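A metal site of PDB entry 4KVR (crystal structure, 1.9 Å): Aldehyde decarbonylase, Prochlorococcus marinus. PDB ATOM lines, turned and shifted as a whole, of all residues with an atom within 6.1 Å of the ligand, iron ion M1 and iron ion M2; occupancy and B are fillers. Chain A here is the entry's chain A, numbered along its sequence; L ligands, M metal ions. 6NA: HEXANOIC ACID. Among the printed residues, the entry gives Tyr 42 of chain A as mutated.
The side-chain amide nitrogen (NE2) of Gln 124 sits close to an oxygen (OXT) of the ligand.
NE2 of His 161 sits close to SD of Met 73 (3.4 Å). The side-chain hydroxyl (OH) of Tyr 136 sits at hydrogen-bond distance from the side-chain carboxylate (OE2) of Glu 46 (2.7 Å). OE2 of Glu 129 lies close to OH of Tyr 53 (2.7 Å). A ring nitrogen (NE2) of His 77 lies within hydrogen-bond range of the side-chain carboxylate of Asp 157 (2.9 Å). O of Gln 124 sits at hydrogen-bond distance from N of Glu 129 (3.2 Å).
Merely in contact with the ligand: Ile 41 (3.9 Å), Gly 45 (3.5 Å), Ala 49 (3.5 Å), Ile 128 (3.4 Å), Phe 131 (3.7 Å), Ala 132 (3.6 Å) and Tyr 136 (3.7 Å). Hydrophobic or aromatic side chains that line the ligand: Ala 49, Ile 128, Phe 131 and Ala 132. The nearest printed residue that does not touch the ligand is Phe 101 (4.1 Å).
The nearest printed residue that does not touch iron ion M1 is His 161 (4.3 Å).
Four residues have an atom within 4 Å of iron ion M2: Glu 74, Glu 129, Glu 158 and His 161.
OE1 of Glu 74 binds iron ion M1 (2.0 Å). Iron ion M1 is bound by the side-chain carboxylate (OE1) of Glu 46 (2.0 Å). The side-chain carboxylate (OE2) of Glu 158 is bound to iron ion M1 (2.1 Å). Iron ion M1 is bound by a ring nitrogen (ND1) of His 77, 2.2 Å away. Iron ion M1 is bound by O of the ligand (2.3 Å). Iron ion M1 is bound by the side-chain carboxylate (OE1) of Glu 158 (2.5 Å). Iron ion M1 has six donor atoms within binding distance.
Iron ion M2 is bound by OE2 of Glu 74 (2.0 Å), OE2 of Glu 129 (2.2 Å), ND1 of His 161 (2.2 Å), OE1 of Glu 158 (2.2 Å), OE1 of Glu 129 (2.3 Å) and OXT of the ligand (2.5 Å).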
ATOM      1  N   ILE A  41       7.550   8.142  -5.016  1.00  0.00           N
ATOM      2  CA  ILE A  41       7.903   9.504  -4.613  1.00  0.00           C
ATOM      3  C   ILE A  41       9.294   9.528  -3.955  1.00  0.00           C
ATOM      4  O   ILE A  41      10.117  10.386  -4.292  1.00  0.00           O
ATOM      5  CB  ILE A  41       6.802  10.122  -3.753  1.00  0.00           C
ATOM      6  CG1 ILE A  41       5.606  10.478  -4.643  1.00  0.00           C
ATOM      7  CG2 ILE A  41       7.334  11.369  -2.997  1.00  0.00           C
ATOM      8  CD1 ILE A  41       4.332  10.773  -3.866  1.00  0.00           C
ATOM      9  N   TYR A  42       9.565   8.578  -3.059  1.00  0.00           N
ATOM     10  CA  TYR A  42      10.889   8.469  -2.458  1.00  0.00           C
ATOM     11  C   TYR A  42      11.963   8.347  -3.548  1.00  0.00           C
ATOM     12  O   TYR A  42      12.924   9.110  -3.585  1.00  0.00           O
ATOM     13  CB  TYR A  42      10.977   7.252  -1.542  1.00  0.00           C
ATOM     14  CG  TYR A  42      10.069   7.259  -0.322  1.00  0.00           C
ATOM     15  CD1 TYR A  42       9.396   8.409   0.082  1.00  0.00           C
ATOM     16  CD2 TYR A  42       9.902   6.107   0.424  1.00  0.00           C
ATOM     17  CE1 TYR A  42       8.576   8.391   1.203  1.00  0.00           C
ATOM     18  CE2 TYR A  42       9.092   6.078   1.537  1.00  0.00           C
ATOM     19  CZ  TYR A  42       8.429   7.214   1.923  1.00  0.00           C
ATOM     20  OH  TYR A  42       7.631   7.146   3.043  1.00  0.00           O
ATOM     21  N   ILE A  43      11.782   7.371  -4.438  1.00  0.00           N
ATOM     22  CA  ILE A  43      12.750   7.118  -5.503  1.00  0.00           C
ATOM     23  C   ILE A  43      12.973   8.338  -6.394  1.00  0.00           C
ATOM     24  O   ILE A  43      14.119   8.758  -6.616  1.00  0.00           O
ATOM     25  CB  ILE A  43      12.336   5.909  -6.349  1.00  0.00           C
ATOM     26  CG1 ILE A  43      12.404   4.642  -5.485  1.00  0.00           C
ATOM     27  CG2 ILE A  43      13.248   5.772  -7.556  1.00  0.00           C
ATOM     28  CD1 ILE A  43      11.703   3.442  -6.125  1.00  0.00           C
ATOM     29  N   GLU A  44      11.888   8.933  -6.871  1.00  0.00           N
ATOM     30  CA  GLU A  44      12.003  10.103  -7.741  1.00  0.00           C
ATOM     31  C   GLU A  44      12.636  11.278  -7.004  1.00  0.00           C
ATOM     32  O   GLU A  44      13.406  12.050  -7.588  1.00  0.00           O
ATOM     33  CB  GLU A  44      10.642  10.501  -8.311  1.00  0.00           C
ATOM     34  CG  GLU A  44      10.653  11.730  -9.231  1.00  0.00           C
ATOM     35  CD  GLU A  44      11.426  11.515 -10.513  1.00  0.00           C
ATOM     36  OE1 GLU A  44      11.689  10.348 -10.889  1.00  0.00           O
ATOM     37  OE2 GLU A  44      11.799  12.506 -11.172  1.00  0.00           O
ATOM     38  N   GLY A  45      12.306  11.415  -5.723  1.00  0.00           N
ATOM     39  CA  GLY A  45      12.823  12.499  -4.907  1.00  0.00           C
ATOM     40  C   GLY A  45      14.338  12.401  -4.788  1.00  0.00           C
ATOM     41  O   GLY A  45      15.041  13.393  -4.924  1.00  0.00           O
ATOM     42  N   GLU A  46      14.824  11.198  -4.550  1.00  0.00           N
ATOM     43  CA  GLU A  46      16.272  10.971  -4.459  1.00  0.00           C
ATOM     44  C   GLU A  46      16.940  11.261  -5.799  1.00  0.00           C
ATOM     45  O   GLU A  46      17.973  11.912  -5.847  1.00  0.00           O
ATOM     46  CB  GLU A  46      16.577   9.535  -4.014  1.00  0.00           C
ATOM     47  CG  GLU A  46      15.971   9.114  -2.682  1.00  0.00           C
ATOM     48  CD  GLU A  46      16.441   9.964  -1.519  1.00  0.00           C
ATOM     49  OE1 GLU A  46      17.492  10.633  -1.642  1.00  0.00           O
ATOM     50  OE2 GLU A  46      15.770   9.938  -0.469  1.00  0.00           O
ATOM     51  N   ALA A  49      17.063  15.042  -6.382  1.00  0.00           N
ATOM     52  CA  ALA A  49      18.056  15.599  -5.468  1.00  0.00           C
ATOM     53  C   ALA A  49      19.460  15.443  -6.059  1.00  0.00           C
ATOM     54  O   ALA A  49      20.235  16.402  -6.108  1.00  0.00           O
ATOM     55  CB  ALA A  49      17.947  14.934  -4.099  1.00  0.00           C
ATOM     56  N   TYR A  53      21.758  18.745  -7.063  1.00  0.00           N
ATOM     57  CA  TYR A  53      23.091  19.027  -6.552  1.00  0.00           C
ATOM     58  C   TYR A  53      24.138  19.142  -7.674  1.00  0.00           C
ATOM     59  O   TYR A  53      24.986  20.028  -7.630  1.00  0.00           O
ATOM     60  CB  TYR A  53      23.486  18.010  -5.473  1.00  0.00           C
ATOM     61  CG  TYR A  53      22.734  18.228  -4.181  1.00  0.00           C
ATOM     62  CD1 TYR A  53      22.742  19.483  -3.581  1.00  0.00           C
ATOM     63  CD2 TYR A  53      21.980  17.213  -3.594  1.00  0.00           C
ATOM     64  CE1 TYR A  53      22.047  19.713  -2.404  1.00  0.00           C
ATOM     65  CE2 TYR A  53      21.265  17.442  -2.416  1.00  0.00           C
ATOM     66  CZ  TYR A  53      21.313  18.706  -1.829  1.00  0.00           C
ATOM     67  OH  TYR A  53      20.627  18.974  -0.669  1.00  0.00           O
ATOM     68  N   MET A  73      25.453  10.437  -2.608  1.00  0.00           N
ATOM     69  CA  MET A  73      24.676   9.944  -1.484  1.00  0.00           C
ATOM     70  C   MET A  73      23.222   9.775  -1.912  1.00  0.00           C
ATOM     71  O   MET A  73      22.583   8.805  -1.548  1.00  0.00           O
ATOM     72  CB  MET A  73      24.703  10.909  -0.285  1.00  0.00           C
ATOM     73  CG  MET A  73      26.073  11.295   0.238  1.00  0.00           C
ATOM     74  SD  MET A  73      25.947  12.481   1.613  1.00  0.00           S
ATOM     75  CE  MET A  73      24.644  11.692   2.533  1.00  0.00           C
ATOM     76  N   GLU A  74      22.723  10.741  -2.686  1.00  0.00           N
ATOM     77  CA  GLU A  74      21.336  10.672  -3.133  1.00  0.00           C
ATOM     78  C   GLU A  74      21.102   9.437  -3.987  1.00  0.00           C
ATOM     79  O   GLU A  74      20.028   8.834  -3.946  1.00  0.00           O
ATOM     80  CB  GLU A  74      20.939  11.935  -3.911  1.00  0.00           C
ATOM     81  CG  GLU A  74      21.109  13.257  -3.132  1.00  0.00           C
ATOM     82  CD  GLU A  74      20.166  13.421  -1.940  1.00  0.00           C
ATOM     83  OE1 GLU A  74      19.610  12.438  -1.433  1.00  0.00           O
ATOM     84  OE2 GLU A  74      19.984  14.582  -1.494  1.00  0.00           O
ATOM     85  N   HIS A  77      20.706   6.554  -1.732  1.00  0.00           N
ATOM     86  CA  HIS A  77      19.365   6.596  -1.162  1.00  0.00           C
ATOM     87  C   HIS A  77      18.361   6.012  -2.172  1.00  0.00           C
ATOM     88  O   HIS A  77      17.477   5.259  -1.803  1.00  0.00           O
ATOM     89  CB  HIS A  77      18.973   8.053  -0.847  1.00  0.00           C
ATOM     90  CG  HIS A  77      19.787   8.696   0.236  1.00  0.00           C
ATOM     91  ND1 HIS A  77      19.737  10.052   0.503  1.00  0.00           N
ATOM     92  CD2 HIS A  77      20.647   8.170   1.141  1.00  0.00           C
ATOM     93  CE1 HIS A  77      20.548  10.326   1.511  1.00  0.00           C
ATOM     94  NE2 HIS A  77      21.105   9.204   1.916  1.00  0.00           N
ATOM     95  N   PHE A 101       6.319  15.841  -8.492  1.00  0.00           N
ATOM     96  CA  PHE A 101       7.460  16.736  -8.331  1.00  0.00           C
ATOM     97  C   PHE A 101       7.512  17.839  -9.392  1.00  0.00           C
ATOM     98  O   PHE A 101       8.321  18.754  -9.291  1.00  0.00           O
ATOM     99  CB  PHE A 101       8.780  15.962  -8.323  1.00  0.00           C
ATOM    100  CG  PHE A 101       9.111  15.333  -6.997  1.00  0.00           C
ATOM    101  CD1 PHE A 101       9.520  16.123  -5.934  1.00  0.00           C
ATOM    102  CD2 PHE A 101       8.969  13.982  -6.805  1.00  0.00           C
ATOM    103  CE1 PHE A 101       9.807  15.548  -4.698  1.00  0.00           C
ATOM    104  CE2 PHE A 101       9.256  13.398  -5.558  1.00  0.00           C
ATOM    105  CZ  PHE A 101       9.675  14.185  -4.515  1.00  0.00           C
ATOM    106  N   GLN A 124      15.987  23.041  -3.046  1.00  0.00           N
ATOM    107  CA  GLN A 124      16.546  21.679  -2.852  1.00  0.00           C
ATOM    108  C   GLN A 124      17.069  21.406  -1.440  1.00  0.00           C
ATOM    109  O   GLN A 124      16.604  20.485  -0.772  1.00  0.00           O
ATOM    110  CB  GLN A 124      17.657  21.360  -3.857  1.00  0.00           C
ATOM    111  CG  GLN A 124      18.367  20.012  -3.555  1.00  0.00           C
ATOM    112  CD  GLN A 124      17.417  18.821  -3.585  1.00  0.00           C
ATOM    113  OE1 GLN A 124      16.613  18.683  -4.514  1.00  0.00           O
ATOM    114  NE2 GLN A 124      17.497  17.957  -2.569  1.00  0.00           N
ATOM    115  N   ILE A 128      13.001  20.684  -0.037  1.00  0.00           N
ATOM    116  CA  ILE A 128      12.951  19.260  -0.383  1.00  0.00           C
ATOM    117  C   ILE A 128      13.623  18.371   0.681  1.00  0.00           C
ATOM    118  O   ILE A 128      13.096  17.316   1.007  1.00  0.00           O
ATOM    119  CB  ILE A 128      13.512  19.015  -1.799  1.00  0.00           C
ATOM    120  CG1 ILE A 128      12.491  19.482  -2.833  1.00  0.00           C
ATOM    121  CG2 ILE A 128      13.775  17.547  -2.039  1.00  0.00           C
ATOM    122  CD1 ILE A 128      13.044  19.556  -4.225  1.00  0.00           C
ATOM    123  N   GLU A 129      14.753  18.805   1.228  1.00  0.00           N
ATOM    124  CA  GLU A 129      15.372  18.028   2.303  1.00  0.00           C
ATOM    125  C   GLU A 129      14.485  17.979   3.542  1.00  0.00           C
ATOM    126  O   GLU A 129      14.364  16.926   4.158  1.00  0.00           O
ATOM    127  CB  GLU A 129      16.766  18.552   2.678  1.00  0.00           C
ATOM    128  CG  GLU A 129      17.757  18.531   1.541  1.00  0.00           C
ATOM    129  CD  GLU A 129      18.216  17.119   1.126  1.00  0.00           C
ATOM    130  OE1 GLU A 129      17.944  16.120   1.835  1.00  0.00           O
ATOM    131  OE2 GLU A 129      18.900  17.026   0.087  1.00  0.00           O
ATOM    132  N   PHE A 131      11.248  18.198   3.527  1.00  0.00           N
ATOM    133  CA  PHE A 131      10.103  17.360   3.173  1.00  0.00           C
ATOM    134  C   PHE A 131      10.523  15.896   3.326  1.00  0.00           C
ATOM    135  O   PHE A 131       9.763  15.061   3.841  1.00  0.00           O
ATOM    136  CB  PHE A 131       9.669  17.653   1.745  1.00  0.00           C
ATOM    137  CG  PHE A 131       8.532  16.805   1.272  1.00  0.00           C
ATOM    138  CD1 PHE A 131       7.220  17.099   1.654  1.00  0.00           C
ATOM    139  CD2 PHE A 131       8.755  15.702   0.459  1.00  0.00           C
ATOM    140  CE1 PHE A 131       6.163  16.300   1.221  1.00  0.00           C
ATOM    141  CE2 PHE A 131       7.708  14.894   0.028  1.00  0.00           C
ATOM    142  CZ  PHE A 131       6.406  15.198   0.408  1.00  0.00           C
ATOM    143  N   ALA A 132      11.743  15.620   2.892  1.00  0.00           N
ATOM    144  CA  ALA A 132      12.299  14.265   2.953  1.00  0.00           C
ATOM    145  C   ALA A 132      12.437  13.794   4.396  1.00  0.00           C
ATOM    146  O   ALA A 132      11.971  12.716   4.756  1.00  0.00           O
ATOM    147  CB  ALA A 132      13.639  14.212   2.263  1.00  0.00           C
ATOM    148  N   ALA A 135       9.042  13.072   5.921  1.00  0.00           N
ATOM    149  CA  ALA A 135       8.473  11.843   5.385  1.00  0.00           C
ATOM    150  C   ALA A 135       9.175  10.637   5.976  1.00  0.00           C
ATOM    151  O   ALA A 135       8.538   9.685   6.439  1.00  0.00           O
ATOM    152  CB  ALA A 135       8.607  11.824   3.883  1.00  0.00           C
ATOM    153  N   TYR A 136      10.504  10.671   5.952  1.00  0.00           N
ATOM    154  CA  TYR A 136      11.293   9.514   6.402  1.00  0.00           C
ATOM    155  C   TYR A 136      11.185   9.302   7.914  1.00  0.00           C
ATOM    156  O   TYR A 136      10.982   8.178   8.370  1.00  0.00           O
ATOM    157  CB  TYR A 136      12.742   9.635   5.934  1.00  0.00           C
ATOM    158  CG  TYR A 136      12.885   9.605   4.424  1.00  0.00           C
ATOM    159  CD1 TYR A 136      12.010   8.874   3.651  1.00  0.00           C
ATOM    160  CD2 TYR A 136      13.896  10.312   3.776  1.00  0.00           C
ATOM    161  CE1 TYR A 136      12.116   8.838   2.285  1.00  0.00           C
ATOM    162  CE2 TYR A 136      14.012  10.281   2.379  1.00  0.00           C
ATOM    163  CZ  TYR A 136      13.107   9.536   1.650  1.00  0.00           C
ATOM    164  OH  TYR A 136      13.184   9.456   0.271  1.00  0.00           O
ATOM    165  N   VAL A 154      19.104   6.585   5.974  1.00  0.00           N
ATOM    166  CA  VAL A 154      18.859   7.751   5.140  1.00  0.00           C
ATOM    167  C   VAL A 154      18.660   9.045   5.939  1.00  0.00           C
ATOM    168  O   VAL A 154      19.238  10.078   5.595  1.00  0.00           O
ATOM    169  CB  VAL A 154      17.657   7.508   4.194  1.00  0.00           C
ATOM    170  CG1 VAL A 154      17.251   8.804   3.492  1.00  0.00           C
ATOM    171  CG2 VAL A 154      17.997   6.430   3.162  1.00  0.00           C
ATOM    172  N   ASP A 157      21.528  11.117   7.014  1.00  0.00           N
ATOM    173  CA  ASP A 157      22.171  11.780   5.892  1.00  0.00           C
ATOM    174  C   ASP A 157      21.539  13.103   5.493  1.00  0.00           C
ATOM    175  O   ASP A 157      22.218  14.034   5.074  1.00  0.00           O
ATOM    176  CB  ASP A 157      22.152  10.864   4.684  1.00  0.00           C
ATOM    177  CG  ASP A 157      23.125   9.716   4.814  1.00  0.00           C
ATOM    178  OD1 ASP A 157      24.124   9.885   5.543  1.00  0.00           O
ATOM    179  OD2 ASP A 157      22.880   8.666   4.202  1.00  0.00           O
ATOM    180  N   GLU A 158      20.217  13.198   5.555  1.00  0.00           N
ATOM    181  CA  GLU A 158      19.616  14.387   4.965  1.00  0.00           C
ATOM    182  C   GLU A 158      19.850  15.635   5.837  1.00  0.00           C
ATOM    183  O   GLU A 158      19.772  16.756   5.354  1.00  0.00           O
ATOM    184  CB  GLU A 158      18.144  14.147   4.540  1.00  0.00           C
ATOM    185  CG  GLU A 158      17.859  12.728   3.923  1.00  0.00           C
ATOM    186  CD  GLU A 158      18.116  12.535   2.390  1.00  0.00           C
ATOM    187  OE1 GLU A 158      18.947  13.225   1.737  1.00  0.00           O
ATOM    188  OE2 GLU A 158      17.479  11.611   1.811  1.00  0.00           O
ATOM    189  N   HIS A 161      22.651  17.334   4.360  1.00  0.00           N
ATOM    190  CA  HIS A 161      22.230  18.105   3.222  1.00  0.00           C
ATOM    191  C   HIS A 161      21.634  19.448   3.672  1.00  0.00           C
ATOM    192  O   HIS A 161      21.947  20.481   3.088  1.00  0.00           O
ATOM    193  CB  HIS A 161      21.245  17.298   2.384  1.00  0.00           C
ATOM    194  CG  HIS A 161      21.819  16.015   1.873  1.00  0.00           C
ATOM    195  ND1 HIS A 161      21.097  15.143   1.083  1.00  0.00           N
ATOM    196  CD2 HIS A 161      23.038  15.451   2.048  1.00  0.00           C
ATOM    197  CE1 HIS A 161      21.849  14.096   0.792  1.00  0.00           C
ATOM    198  NE2 HIS A 161      23.036  14.253   1.367  1.00  0.00           N
HETATM  199  CA  6NA L   1      14.817  14.351  -1.556  1.00  0.00           C
HETATM  200  C   6NA L   1      16.181  14.252  -0.957  1.00  0.00           C
HETATM  201  O   6NA L   1      16.625  13.131  -0.652  1.00  0.00           O
HETATM  202  CB  6NA L   1      13.953  13.186  -1.164  1.00  0.00           C
HETATM  203  CG  6NA L   1      12.521  13.638  -1.134  1.00  0.00           C
HETATM  204  CD  6NA L   1      11.608  12.464  -1.299  1.00  0.00           C
HETATM  205  C6  6NA L   1      10.525  12.493  -0.274  1.00  0.00           C
HETATM  206  OXT 6NA L   1      16.879  15.276  -0.743  1.00  0.00           O
HETATM  207 FE    FE M   1      18.353  11.689  -0.125  1.00  0.00          FE
HETATM  208 FE    FE M   2      19.079  14.865   0.306  1.00  0.00          FE
